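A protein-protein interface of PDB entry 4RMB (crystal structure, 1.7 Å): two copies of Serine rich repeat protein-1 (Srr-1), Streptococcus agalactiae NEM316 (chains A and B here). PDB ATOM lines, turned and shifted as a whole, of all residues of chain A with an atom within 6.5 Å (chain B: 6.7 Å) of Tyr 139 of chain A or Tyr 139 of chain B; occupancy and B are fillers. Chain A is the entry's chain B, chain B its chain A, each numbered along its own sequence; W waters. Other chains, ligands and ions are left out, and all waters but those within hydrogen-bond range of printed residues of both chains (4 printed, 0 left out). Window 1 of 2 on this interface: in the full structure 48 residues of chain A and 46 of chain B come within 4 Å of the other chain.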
ATOM      1  N   TYR A  14      -7.485   3.194  14.936  1.00  0.00           N
ATOM      2  CA  TYR A  14      -8.112   2.092  15.649  1.00  0.00           C
ATOM      3  C   TYR A  14      -9.575   2.501  15.708  1.00  0.00           C
ATOM      4  O   TYR A  14      -9.927   3.473  16.376  1.00  0.00           O
ATOM      5  CB  TYR A  14      -7.519   1.979  17.049  1.00  0.00           C
ATOM      6  CG  TYR A  14      -8.157   0.911  17.898  1.00  0.00           C
ATOM      7  CD1 TYR A  14      -8.097  -0.431  17.525  1.00  0.00           C
ATOM      8  CD2 TYR A  14      -8.827   1.241  19.071  1.00  0.00           C
ATOM      9  CE1 TYR A  14      -8.694  -1.420  18.302  1.00  0.00           C
ATOM     10  CE2 TYR A  14      -9.425   0.262  19.855  1.00  0.00           C
ATOM     11  CZ  TYR A  14      -9.357  -1.061  19.464  1.00  0.00           C
ATOM     12  OH  TYR A  14      -9.968  -2.023  20.223  1.00  0.00           O
ATOM     13  N   ASP A  41      -2.947  -4.096  26.115  1.00  0.00           N
ATOM     14  CA  ASP A  41      -2.624  -5.212  26.996  1.00  0.00           C
ATOM     15  C   ASP A  41      -1.124  -5.359  27.213  1.00  0.00           C
ATOM     16  O   ASP A  41      -0.473  -4.456  27.741  1.00  0.00           O
ATOM     17  CB  ASP A  41      -3.199  -6.506  26.423  1.00  0.00           C
ATOM     18  CG  ASP A  41      -4.699  -6.435  26.232  1.00  0.00           C
ATOM     19  OD1 ASP A  41      -5.420  -6.267  27.240  1.00  0.00           O
ATOM     20  OD2 ASP A  41      -5.155  -6.543  25.073  1.00  0.00           O
ATOM     21  N   GLY A 120       1.239  -4.203  18.772  1.00  0.00           N
ATOM     22  CA  GLY A 120       0.651  -4.392  20.081  1.00  0.00           C
ATOM     23  C   GLY A 120      -0.818  -4.722  19.948  1.00  0.00           C
ATOM     24  O   GLY A 120      -1.339  -4.834  18.841  1.00  0.00           O
ATOM     25  N   VAL A 121      -1.492  -4.875  21.077  1.00  0.00           N
ATOM     26  CA  VAL A 121      -2.906  -5.204  21.060  1.00  0.00           C
ATOM     27  C   VAL A 121      -3.725  -4.181  21.828  1.00  0.00           C
ATOM     28  O   VAL A 121      -3.432  -3.859  22.981  1.00  0.00           O
ATOM     29  CB  VAL A 121      -3.162  -6.595  21.666  1.00  0.00           C
ATOM     30  CG1 VAL A 121      -4.646  -6.935  21.594  1.00  0.00           C
ATOM     31  CG2 VAL A 121      -2.338  -7.642  20.923  1.00  0.00           C
ATOM     32  N   LEU A 122      -4.746  -3.656  21.168  1.00  0.00           N
ATOM     33  CA  LEU A 122      -5.627  -2.688  21.799  1.00  0.00           C
ATOM     34  C   LEU A 122      -6.938  -3.399  22.111  1.00  0.00           C
ATOM     35  O   LEU A 122      -7.228  -4.462  21.559  1.00  0.00           O
ATOM     36  CB  LEU A 122      -5.898  -1.527  20.843  1.00  0.00           C
ATOM     37  CG  LEU A 122      -4.676  -0.663  20.524  1.00  0.00           C
ATOM     38  CD1 LEU A 122      -4.981   0.292  19.380  1.00  0.00           C
ATOM     39  CD2 LEU A 122      -4.274   0.097  21.781  1.00  0.00           C
ATOM     40  N   TYR A 123      -7.720  -2.830  23.016  1.00  0.00           N
ATOM     41  CA  TYR A 123      -9.018  -3.411  23.326  1.00  0.00           C
ATOM     42  C   TYR A 123     -10.027  -2.283  23.443  1.00  0.00           C
ATOM     43  O   TYR A 123      -9.661  -1.133  23.682  1.00  0.00           O
ATOM     44  CB  TYR A 123      -8.979  -4.221  24.635  1.00  0.00           C
ATOM     45  CG  TYR A 123      -8.920  -3.404  25.914  1.00  0.00           C
ATOM     46  CD1 TYR A 123     -10.059  -2.767  26.417  1.00  0.00           C
ATOM     47  CD2 TYR A 123      -7.730  -3.280  26.624  1.00  0.00           C
ATOM     48  CE1 TYR A 123     -10.010  -2.028  27.595  1.00  0.00           C
ATOM     49  CE2 TYR A 123      -7.667  -2.542  27.806  1.00  0.00           C
ATOM     50  CZ  TYR A 123      -8.812  -1.919  28.283  1.00  0.00           C
ATOM     51  OH  TYR A 123      -8.757  -1.181  29.438  1.00  0.00           O
ATOM     52  N   SER A 124     -11.293  -2.625  23.238  1.00  0.00           N
ATOM     53  CA  SER A 124     -12.394  -1.680  23.345  1.00  0.00           C
ATOM     54  C   SER A 124     -13.514  -2.393  24.087  1.00  0.00           C
ATOM     55  O   SER A 124     -13.685  -3.604  23.956  1.00  0.00           O
ATOM     56  CB  SER A 124     -12.908  -1.262  21.966  1.00  0.00           C
ATOM     57  OG  SER A 124     -11.947  -0.517  21.248  1.00  0.00           O
ATOM     58  N   TYR A 137     -13.465  -6.396  23.437  1.00  0.00           N
ATOM     59  CA  TYR A 137     -12.902  -6.906  22.185  1.00  0.00           C
ATOM     60  C   TYR A 137     -11.447  -6.479  22.081  1.00  0.00           C
ATOM     61  O   TYR A 137     -11.093  -5.392  22.504  1.00  0.00           O
ATOM     62  CB  TYR A 137     -13.671  -6.339  20.995  1.00  0.00           C
ATOM     63  CG  TYR A 137     -15.163  -6.530  21.104  1.00  0.00           C
ATOM     64  CD1 TYR A 137     -15.927  -5.732  21.954  1.00  0.00           C
ATOM     65  CD2 TYR A 137     -15.804  -7.536  20.387  1.00  0.00           C
ATOM     66  CE1 TYR A 137     -17.296  -5.935  22.087  1.00  0.00           C
ATOM     67  CE2 TYR A 137     -17.169  -7.747  20.511  1.00  0.00           C
ATOM     68  CZ  TYR A 137     -17.907  -6.944  21.364  1.00  0.00           C
ATOM     69  OH  TYR A 137     -19.259  -7.161  21.480  1.00  0.00           O
ATOM     70  N   SER A 138     -10.597  -7.328  21.516  1.00  0.00           N
ATOM     71  CA  SER A 138      -9.191  -6.968  21.396  1.00  0.00           C
ATOM     72  C   SER A 138      -8.721  -7.132  19.953  1.00  0.00           C
ATOM     73  O   SER A 138      -9.214  -7.992  19.223  1.00  0.00           O
ATOM     74  CB  SER A 138      -8.344  -7.824  22.339  1.00  0.00           C
ATOM     75  OG  SER A 138      -8.366  -9.188  21.959  1.00  0.00           O
ATOM     76  N   TYR A 139      -7.764  -6.309  19.542  1.00  0.00           N
ATOM     77  CA  TYR A 139      -7.266  -6.364  18.171  1.00  0.00           C
ATOM     78  C   TYR A 139      -5.847  -5.839  18.108  1.00  0.00           C
ATOM     79  O   TYR A 139      -5.518  -4.826  18.716  1.00  0.00           O
ATOM     80  CB  TYR A 139      -8.163  -5.514  17.261  1.00  0.00           C
ATOM     81  CG  TYR A 139      -7.886  -5.655  15.779  1.00  0.00           C
ATOM     82  CD1 TYR A 139      -6.702  -5.183  15.213  1.00  0.00           C
ATOM     83  CD2 TYR A 139      -8.814  -6.272  14.942  1.00  0.00           C
ATOM     84  CE1 TYR A 139      -6.451  -5.330  13.844  1.00  0.00           C
ATOM     85  CE2 TYR A 139      -8.575  -6.421  13.579  1.00  0.00           C
ATOM     86  CZ  TYR A 139      -7.391  -5.949  13.038  1.00  0.00           C
ATOM     87  OH  TYR A 139      -7.155  -6.108  11.691  1.00  0.00           O
ATOM     88  N   GLY A 140      -4.996  -6.514  17.354  1.00  0.00           N
ATOM     89  CA  GLY A 140      -3.638  -6.032  17.260  1.00  0.00           C
ATOM     90  C   GLY A 140      -2.827  -6.777  16.230  1.00  0.00           C
ATOM     91  O   GLY A 140      -3.299  -7.737  15.628  1.00  0.00           O
ATOM     92  N   HIS A 141      -1.613  -6.296  16.003  1.00  0.00           N
ATOM     93  CA  HIS A 141      -0.716  -6.939  15.061  1.00  0.00           C
ATOM     94  C   HIS A 141       0.705  -6.763  15.543  1.00  0.00           C
ATOM     95  O   HIS A 141       0.999  -5.871  16.337  1.00  0.00           O
ATOM     96  CB  HIS A 141      -0.892  -6.380  13.635  1.00  0.00           C
ATOM     97  CG  HIS A 141      -0.659  -4.905  13.502  1.00  0.00           C
ATOM     98  ND1 HIS A 141       0.566  -4.316  13.730  1.00  0.00           N
ATOM     99  CD2 HIS A 141      -1.486  -3.910  13.102  1.00  0.00           C
ATOM    100  CE1 HIS A 141       0.484  -3.022  13.474  1.00  0.00           C
ATOM    101  NE2 HIS A 141      -0.751  -2.749  13.090  1.00  0.00           N
ATOM    102  N   LYS A 155       1.602  -3.750   4.891  1.00  0.00           N
ATOM    103  CA  LYS A 155       0.609  -4.554   5.579  1.00  0.00           C
ATOM    104  C   LYS A 155       0.475  -5.866   4.807  1.00  0.00           C
ATOM    105  O   LYS A 155      -0.075  -5.894   3.707  1.00  0.00           O
ATOM    106  CB  LYS A 155      -0.727  -3.799   5.613  1.00  0.00           C
ATOM    107  CG  LYS A 155      -1.746  -4.391   6.562  1.00  0.00           C
ATOM    108  CD  LYS A 155      -2.955  -3.481   6.704  1.00  0.00           C
ATOM    109  CE  LYS A 155      -3.947  -4.043   7.707  1.00  0.00           C
ATOM    110  NZ  LYS A 155      -5.075  -3.094   7.925  1.00  0.00           N
ATOM    111  N   LEU A 157      -1.238  -8.524   5.742  1.00  0.00           N
ATOM    112  CA  LEU A 157      -2.579  -9.067   5.854  1.00  0.00           C
ATOM    113  C   LEU A 157      -3.424  -8.170   6.731  1.00  0.00           C
ATOM    114  O   LEU A 157      -2.940  -7.197   7.308  1.00  0.00           O
ATOM    115  CB  LEU A 157      -2.558 -10.470   6.482  1.00  0.00           C
ATOM    116  CG  LEU A 157      -2.233 -10.549   7.982  1.00  0.00           C
ATOM    117  CD1 LEU A 157      -2.693 -11.899   8.556  1.00  0.00           C
ATOM    118  CD2 LEU A 157      -0.746 -10.335   8.193  1.00  0.00           C
ATOM    119  N   SER A 158      -4.696  -8.521   6.820  1.00  0.00           N
ATOM    120  CA  SER A 158      -5.636  -7.814   7.647  1.00  0.00           C
ATOM    121  C   SER A 158      -6.549  -8.888   8.200  1.00  0.00           C
ATOM    122  O   SER A 158      -6.784  -9.920   7.578  1.00  0.00           O
ATOM    123  CB  SER A 158      -6.448  -6.823   6.816  1.00  0.00           C
ATOM    124  OG  SER A 158      -7.334  -6.088   7.632  1.00  0.00           O
ATOM    125  N   LEU A 159      -7.071  -8.651   9.398  1.00  0.00           N
ATOM    126  CA  LEU A 159      -7.981  -9.601  10.031  1.00  0.00           C
ATOM    127  C   LEU A 159      -9.208  -8.873  10.559  1.00  0.00           C
ATOM    128  O   LEU A 159      -9.089  -7.806  11.161  1.00  0.00           O
ATOM    129  CB  LEU A 159      -7.277 -10.344  11.168  1.00  0.00           C
ATOM    130  CG  LEU A 159      -8.158 -11.243  12.036  1.00  0.00           C
ATOM    131  CD1 LEU A 159      -8.479 -12.542  11.312  1.00  0.00           C
ATOM    132  CD2 LEU A 159      -7.491 -11.520  13.375  1.00  0.00           C
ATOM    133  N   GLU A 160     -10.390  -9.441  10.334  1.00  0.00           N
ATOM    134  CA  GLU A 160     -11.608  -8.774  10.764  1.00  0.00           C
ATOM    135  C   GLU A 160     -12.648  -9.800  11.095  1.00  0.00           C
ATOM    136  O   GLU A 160     -12.628 -10.921  10.588  1.00  0.00           O
ATOM    137  CB  GLU A 160     -12.121  -7.804   9.700  1.00  0.00           C
ATOM    138  CG  GLU A 160     -12.472  -8.395   8.363  1.00  0.00           C
ATOM    139  CD  GLU A 160     -12.803  -7.322   7.353  1.00  0.00           C
ATOM    140  OE1 GLU A 160     -13.583  -7.605   6.423  1.00  0.00           O
ATOM    141  OE2 GLU A 160     -12.279  -6.197   7.487  1.00  0.00           O
ATOM    142  N   HIS A 161     -13.522  -9.413  12.004  1.00  0.00           N
ATOM    143  CA  HIS A 161     -14.584 -10.275  12.434  1.00  0.00           C
ATOM    144  C   HIS A 161     -15.822  -9.811  11.704  1.00  0.00           C
ATOM    145  O   HIS A 161     -16.080  -8.621  11.600  1.00  0.00           O
ATOM    146  CB  HIS A 161     -14.743 -10.172  13.949  1.00  0.00           C
ATOM    147  CG  HIS A 161     -15.959 -10.856  14.476  1.00  0.00           C
ATOM    148  ND1 HIS A 161     -17.173 -10.211  14.608  1.00  0.00           N
ATOM    149  CD2 HIS A 161     -16.162 -12.126  14.886  1.00  0.00           C
ATOM    150  CE1 HIS A 161     -18.065 -11.056  15.080  1.00  0.00           C
ATOM    151  NE2 HIS A 161     -17.479 -12.229  15.258  1.00  0.00           N
ATOM    152  N   TYR B  14     -14.411 -15.252  10.552  1.00  0.00           N
ATOM    153  CA  TYR B  14     -13.224 -14.417  10.608  1.00  0.00           C
ATOM    154  C   TYR B  14     -12.699 -14.300   9.192  1.00  0.00           C
ATOM    155  O   TYR B  14     -12.534 -15.304   8.494  1.00  0.00           O
ATOM    156  CB  TYR B  14     -12.168 -15.041  11.520  1.00  0.00           C
ATOM    157  CG  TYR B  14     -12.570 -15.057  12.975  1.00  0.00           C
ATOM    158  CD1 TYR B  14     -13.497 -15.979  13.454  1.00  0.00           C
ATOM    159  CD2 TYR B  14     -12.033 -14.134  13.871  1.00  0.00           C
ATOM    160  CE1 TYR B  14     -13.879 -15.985  14.794  1.00  0.00           C
ATOM    161  CE2 TYR B  14     -12.405 -14.129  15.211  1.00  0.00           C
ATOM    162  CZ  TYR B  14     -13.328 -15.056  15.667  1.00  0.00           C
ATOM    163  OH  TYR B  14     -13.688 -15.056  16.994  1.00  0.00           O
ATOM    164  N   GLY B 120     -12.834 -15.940  22.900  1.00  0.00           N
ATOM    165  CA  GLY B 120     -11.406 -16.194  22.948  1.00  0.00           C
ATOM    166  C   GLY B 120     -10.648 -15.368  21.928  1.00  0.00           C
ATOM    167  O   GLY B 120     -11.224 -14.481  21.295  1.00  0.00           O
ATOM    168  N   VAL B 121      -9.364 -15.673  21.754  1.00  0.00           N
ATOM    169  CA  VAL B 121      -8.505 -14.942  20.826  1.00  0.00           C
ATOM    170  C   VAL B 121      -8.011 -15.797  19.662  1.00  0.00           C
ATOM    171  O   VAL B 121      -7.404 -16.849  19.867  1.00  0.00           O
ATOM    172  CB  VAL B 121      -7.262 -14.382  21.559  1.00  0.00           C
ATOM    173  CG1 VAL B 121      -6.343 -13.675  20.572  1.00  0.00           C
ATOM    174  CG2 VAL B 121      -7.690 -13.434  22.668  1.00  0.00           C
ATOM    175  N   LEU B 122      -8.274 -15.337  18.443  1.00  0.00           N
ATOM    176  CA  LEU B 122      -7.830 -16.050  17.252  1.00  0.00           C
ATOM    177  C   LEU B 122      -6.765 -15.199  16.565  1.00  0.00           C
ATOM    178  O   LEU B 122      -6.816 -13.969  16.625  1.00  0.00           O
ATOM    179  CB  LEU B 122      -8.995 -16.250  16.290  1.00  0.00           C
ATOM    180  CG  LEU B 122      -8.759 -17.335  15.239  1.00  0.00           C
ATOM    181  CD1 LEU B 122      -9.451 -18.615  15.689  1.00  0.00           C
ATOM    182  CD2 LEU B 122      -9.301 -16.882  13.900  1.00  0.00           C
ATOM    183  N   TYR B 123      -5.789 -15.839  15.930  1.00  0.00           N
ATOM    184  CA  TYR B 123      -4.757 -15.081  15.227  1.00  0.00           C
ATOM    185  C   TYR B 123      -4.633 -15.574  13.787  1.00  0.00           C
ATOM    186  O   TYR B 123      -5.041 -16.688  13.468  1.00  0.00           O
ATOM    187  CB  TYR B 123      -3.399 -15.194  15.945  1.00  0.00           C
ATOM    188  CG  TYR B 123      -2.738 -16.554  15.889  1.00  0.00           C
ATOM    189  CD1 TYR B 123      -2.104 -16.996  14.727  1.00  0.00           C
ATOM    190  CD2 TYR B 123      -2.750 -17.402  16.999  1.00  0.00           C
ATOM    191  CE1 TYR B 123      -1.496 -18.253  14.671  1.00  0.00           C
ATOM    192  CE2 TYR B 123      -2.146 -18.659  16.952  1.00  0.00           C
ATOM    193  CZ  TYR B 123      -1.523 -19.076  15.786  1.00  0.00           C
ATOM    194  OH  TYR B 123      -0.931 -20.320  15.724  1.00  0.00           O
ATOM    195  N   SER B 124      -4.112 -14.716  12.916  1.00  0.00           N
ATOM    196  CA  SER B 124      -3.884 -15.060  11.509  1.00  0.00           C
ATOM    197  C   SER B 124      -2.523 -14.496  11.165  1.00  0.00           C
ATOM    198  O   SER B 124      -2.137 -13.444  11.681  1.00  0.00           O
ATOM    199  CB  SER B 124      -4.920 -14.414  10.581  1.00  0.00           C
ATOM    200  OG  SER B 124      -6.205 -14.973  10.747  1.00  0.00           O
ATOM    201  N   TYR B 137      -1.714 -11.030  13.126  1.00  0.00           N
ATOM    202  CA  TYR B 137      -2.815 -10.194  13.608  1.00  0.00           C
ATOM    203  C   TYR B 137      -3.629 -11.040  14.576  1.00  0.00           C
ATOM    204  O   TYR B 137      -3.766 -12.243  14.387  1.00  0.00           O
ATOM    205  CB  TYR B 137      -3.719  -9.750  12.454  1.00  0.00           C
ATOM    206  CG  TYR B 137      -3.241  -8.505  11.753  1.00  0.00           C
ATOM    207  CD1 TYR B 137      -2.035  -8.491  11.053  1.00  0.00           C
ATOM    208  CD2 TYR B 137      -3.980  -7.325  11.818  1.00  0.00           C
ATOM    209  CE1 TYR B 137      -1.577  -7.325  10.439  1.00  0.00           C
ATOM    210  CE2 TYR B 137      -3.531  -6.159  11.210  1.00  0.00           C
ATOM    211  CZ  TYR B 137      -2.328  -6.167  10.525  1.00  0.00           C
ATOM    212  OH  TYR B 137      -1.874  -5.010   9.941  1.00  0.00           O
ATOM    213  N   SER B 138      -4.173 -10.415  15.614  1.00  0.00           N
ATOM    214  CA  SER B 138      -4.961 -11.151  16.600  1.00  0.00           C
ATOM    215  C   SER B 138      -6.292 -10.459  16.862  1.00  0.00           C
ATOM    216  O   SER B 138      -6.358  -9.231  16.906  1.00  0.00           O
ATOM    217  CB  SER B 138      -4.192 -11.257  17.923  1.00  0.00           C
ATOM    218  OG  SER B 138      -3.025 -12.051  17.789  1.00  0.00           O
ATOM    219  N   TYR B 139      -7.349 -11.246  17.027  1.00  0.00           N
ATOM    220  CA  TYR B 139      -8.663 -10.680  17.313  1.00  0.00           C
ATOM    221  C   TYR B 139      -9.341 -11.457  18.432  1.00  0.00           C
ATOM    222  O   TYR B 139      -9.421 -12.684  18.393  1.00  0.00           O
ATOM    223  CB  TYR B 139      -9.548 -10.686  16.063  1.00  0.00           C
ATOM    224  CG  TYR B 139     -10.950 -10.182  16.336  1.00  0.00           C
ATOM    225  CD1 TYR B 139     -11.905 -11.014  16.920  1.00  0.00           C
ATOM    226  CD2 TYR B 139     -11.306  -8.862  16.057  1.00  0.00           C
ATOM    227  CE1 TYR B 139     -13.178 -10.551  17.220  1.00  0.00           C
ATOM    228  CE2 TYR B 139     -12.586  -8.383  16.359  1.00  0.00           C
ATOM    229  CZ  TYR B 139     -13.513  -9.239  16.939  1.00  0.00           C
ATOM    230  OH  TYR B 139     -14.790  -8.805  17.222  1.00  0.00           O
ATOM    231  N   GLY B 140      -9.839 -10.745  19.434  1.00  0.00           N
ATOM    232  CA  GLY B 140     -10.480 -11.431  20.535  1.00  0.00           C
ATOM    233  C   GLY B 140     -11.761 -10.807  21.039  1.00  0.00           C
ATOM    234  O   GLY B 140     -11.994  -9.611  20.894  1.00  0.00           O
ATOM    235  N   HIS B 141     -12.613 -11.641  21.618  1.00  0.00           N
ATOM    236  CA  HIS B 141     -13.869 -11.171  22.181  1.00  0.00           C
ATOM    237  C   HIS B 141     -14.167 -11.946  23.449  1.00  0.00           C
ATOM    238  O   HIS B 141     -14.054 -13.167  23.482  1.00  0.00           O
ATOM    239  CB  HIS B 141     -15.024 -11.346  21.196  1.00  0.00           C
ATOM    240  CG  HIS B 141     -16.376 -11.191  21.827  1.00  0.00           C
ATOM    241  ND1 HIS B 141     -16.686 -10.148  22.671  1.00  0.00           N
ATOM    242  CD2 HIS B 141     -17.492 -11.954  21.744  1.00  0.00           C
ATOM    243  CE1 HIS B 141     -17.935 -10.273  23.084  1.00  0.00           C
ATOM    244  NE2 HIS B 141     -18.447 -11.360  22.536  1.00  0.00           N
ATOM    245  N   ALA B 152     -19.930  -4.429  20.124  1.00  0.00           N
ATOM    246  CA  ALA B 152     -19.094  -3.529  19.351  1.00  0.00           C
ATOM    247  C   ALA B 152     -18.289  -4.357  18.363  1.00  0.00           C
ATOM    248  O   ALA B 152     -18.310  -5.592  18.410  1.00  0.00           O
ATOM    249  CB  ALA B 152     -18.142  -2.763  20.280  1.00  0.00           C
ATOM    250  N   GLU B 153     -17.602  -3.665  17.464  1.00  0.00           N
ATOM    251  CA  GLU B 153     -16.742  -4.295  16.476  1.00  0.00           C
ATOM    252  C   GLU B 153     -15.517  -3.401  16.379  1.00  0.00           C
ATOM    253  O   GLU B 153     -15.637  -2.180  16.460  1.00  0.00           O
ATOM    254  CB  GLU B 153     -17.432  -4.390  15.114  1.00  0.00           C
ATOM    255  CG  GLU B 153     -16.726  -5.361  14.199  1.00  0.00           C
ATOM    256  CD  GLU B 153     -16.499  -6.700  14.876  1.00  0.00           C
ATOM    257  OE1 GLU B 153     -17.453  -7.500  14.950  1.00  0.00           O
ATOM    258  OE2 GLU B 153     -15.370  -6.937  15.357  1.00  0.00           O
ATOM    259  N   ILE B 154     -14.339  -3.997  16.216  1.00  0.00           N
ATOM    260  CA  ILE B 154     -13.117  -3.207  16.145  1.00  0.00           C
ATOM    261  C   ILE B 154     -12.194  -3.633  15.017  1.00  0.00           C
ATOM    262  O   ILE B 154     -12.282  -4.751  14.513  1.00  0.00           O
ATOM    263  CB  ILE B 154     -12.325  -3.276  17.472  1.00  0.00           C
ATOM    264  CG1 ILE B 154     -11.938  -4.728  17.782  1.00  0.00           C
ATOM    265  CG2 ILE B 154     -13.176  -2.712  18.615  1.00  0.00           C
ATOM    266  CD1 ILE B 154     -11.061  -4.879  19.010  1.00  0.00           C
ATOM    267  N   LYS B 155     -11.306  -2.726  14.628  1.00  0.00           N
ATOM    268  CA  LYS B 155     -10.353  -3.003  13.569  1.00  0.00           C
ATOM    269  C   LYS B 155      -9.351  -1.863  13.450  1.00  0.00           C
ATOM    270  O   LYS B 155      -9.646  -0.724  13.817  1.00  0.00           O
ATOM    271  CB  LYS B 155     -11.082  -3.179  12.237  1.00  0.00           C
ATOM    272  CG  LYS B 155     -10.167  -3.582  11.096  1.00  0.00           C
ATOM    273  CD  LYS B 155     -10.931  -3.757   9.796  1.00  0.00           C
ATOM    274  CE  LYS B 155      -9.985  -4.119   8.661  1.00  0.00           C
ATOM    275  NZ  LYS B 155     -10.702  -4.232   7.365  1.00  0.00           N
ATOM    276  N   LEU B 156      -8.162  -2.186  12.952  1.00  0.00           N
ATOM    277  CA  LEU B 156      -7.112  -1.197  12.738  1.00  0.00           C
ATOM    278  C   LEU B 156      -7.004  -0.978  11.236  1.00  0.00           C
ATOM    279  O   LEU B 156      -6.836  -1.936  10.482  1.00  0.00           O
ATOM    280  CB  LEU B 156      -5.769  -1.707  13.259  1.00  0.00           C
ATOM    281  CG  LEU B 156      -5.383  -1.384  14.700  1.00  0.00           C
ATOM    282  CD1 LEU B 156      -4.092  -2.108  15.054  1.00  0.00           C
ATOM    283  CD2 LEU B 156      -5.207   0.119  14.855  1.00  0.00           C
ATOM    284  N   LEU B 157      -7.101   0.271  10.795  1.00  0.00           N
ATOM    285  CA  LEU B 157      -7.012   0.557   9.370  1.00  0.00           C
ATOM    286  C   LEU B 157      -6.371   1.907   9.073  1.00  0.00           C
ATOM    287  O   LEU B 157      -6.402   2.819   9.900  1.00  0.00           O
ATOM    288  CB  LEU B 157      -8.396   0.493   8.745  1.00  0.00           C
HETATM  289  O   HOH W   1      -6.438  -4.312   9.791  1.00  0.00           O
HETATM  290  O   HOH W   2     -16.715 -10.494  18.125  1.00  0.00           O
HETATM  291  O   HOH W   3      -3.468  -2.818  10.718  1.00  0.00           O
HETATM  292  O   HOH W   4     -13.249  -6.592  12.824  1.00  0.00           O
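NZ of Lys 155 of chain A lies within hydrogen-bond range of O of Leu 156 of chain B (3.3 Å).
The side-chain amino group of Lys 155 of chain B lies within salt-bridge range of the side-chain carboxylate of Glu 160 of chain A.
The side-chain carboxylate (OE1) of Glu 153 of chain B sits at hydrogen-bond distance from a ring nitrogen (ND1) of His 161 of chain A.
O of Gly 140 of chain B sits at hydrogen-bond distance from N of Ser 138 of chain A, at 2.7 Å.
N of Ala 152 of chain B sits at hydrogen-bond distance from OH of Tyr 137 of chain A.
N of Ser 138 of chain B sits at hydrogen-bond distance from O of Gly 140 of chain A (2.8 Å).
O of Leu 122 of chain B sits at hydrogen-bond distance from N of Tyr 139 of chain B (2.8 Å).
The side-chain carboxylate (OE2) of Glu 153 of chain B lies within hydrogen-bond range of the side-chain hydroxyl (OH) of Tyr 139 of chain B (2.7 Å).
The backbone NH of Gly 120 of chain B sits at hydrogen-bond distance from the backbone carbonyl oxygen of His 141 of chain B (3.1 Å).
OH of Tyr 139 of chain A is in hydrogen-bond range of O of Leu 159 of chain A, 2.6 Å away.
The backbone NH (N) of Tyr 137 of chain B sits at hydrogen-bond distance from the backbone carbonyl oxygen (O) of Ser 124 of chain B (2.8 Å).
CD1 of Ile 154 of chain B touches OH of Tyr 14 of chain A, 3.3 Å away.
Leu 156 of chain B touches Tyr 14 of chain A (CD2 to CA, 3.6 Å).
Ser 138 of chain A touches Ser 138 of chain B (O to O, 3.9 Å).
O of Ser 138 of chain A touches CA of Tyr 139 of chain B (3.3 Å).
Tyr 137 of chain B touches Tyr 139 of chain A (CD2 to OH, 3.4 Å).
Tyr 139 of chain A touches Ile 154 of chain B (CB to CD1, 3.4 Å).
Tyr 137 of chain B touches Gly 140 of chain A (CA to O, 3.2 Å).
Lys 155 of chain A touches Tyr 137 of chain B (CE to OH, 3.2 Å).
CB of Leu 159 of chain A touches CB of Tyr 137 of chain B, 3.8 Å away.
Tyr 123 of chain A touches none of the printed residues of chain B.
Of the printed residues of chain B, Ser 124 of chain A touches Ile 154 (3.6 Å).
Of the printed residues of chain B, Tyr 137 of chain A touches Tyr 139, Gly 140, His 141, Ala 152 and Ile 154.
Of chain B, only Tyr 137, Ser 138, Tyr 139, Ile 154, Lys 155 and Leu 156 come within 4 Å of Tyr 139 of chain A.
Of the printed residues of chain B, Gly 140 of chain A touches Tyr 137 and Ser 138.
Of the printed residues of chain B, Leu 157 of chain A touches Ser 124 (3.5 Å) and Tyr 137 (3.4 Å).
Tyr 139 of chain B touches five residues of chain A.
Of the printed residues of chain A, Ala 152 of chain B touches Tyr 137 (3.1 Å).
The nearest residue of chain A that does not touch Tyr 139 of chain B is Glu 160 of chain A (5.2 Å).
Of the 18 printed residues of chain A, 13 touch a printed residue of chain B.
Hydrophobic or aromatic side chains of chain A that line the printed part of chain B: Tyr 14, Tyr 137, Tyr 139, His 141, Leu 157, Leu 159 and His 161.
Of the 17 printed residues of chain B, 12 touch a printed residue of chain A.
Printed residues of chain B that touch a printed residue of chain A: Tyr 14, Ser 124, Tyr 137, Ser 138, Tyr 139, Gly 140, His 141, Ala 152, Glu 153, Ile 154, Lys 155 and Leu 156.
Among the printed residues, Asp or Glu carboxylates within 4 Å of a Lys or Arg side-chain nitrogen of the other chain: Glu 160 of chain A with Lys 155 of chain B.
Tyr 14 of chain A touches Lys 155 of chain B, but with the chains exchanged Lys 155 of chain A does not touch Tyr 14 of chain B (13.6 Å).
Tyr 139 of chain A touches Lys 155 of chain B, but with the chains exchanged Lys 155 of chain A does not touch Tyr 139 of chain B (11.8 Å).
Leu 157 of chain A touches Tyr 137 of chain B, but with the chains exchanged Tyr 137 of chain A does not touch Leu 157 of chain B (13.6 Å).
Positions printed for both chains: 14, 120, 121, 122, 123, 124, 137, 138, 139, 140, 141, 155 and 157.
Water W4 lies within hydrogen-bond range of O of Ile 154 of chain B (2.7 Å), N of His 161 of chain A (3.0 Å) and OE2 of Glu 153 of chain B (3.3 Å).
Water W2 bridges the side-chain hydroxyl (OH) of Tyr 139 of chain B (2.7 Å) and a ring nitrogen (NE2) of His 161 of chain A (3.4 Å).
Water W3 lies within hydrogen-bond range of OH of Tyr 137 of chain B (2.8 Å), NZ of Lys 155 of chain A (3.2 Å) and O of Leu 156 of chain B (3.5 Å).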
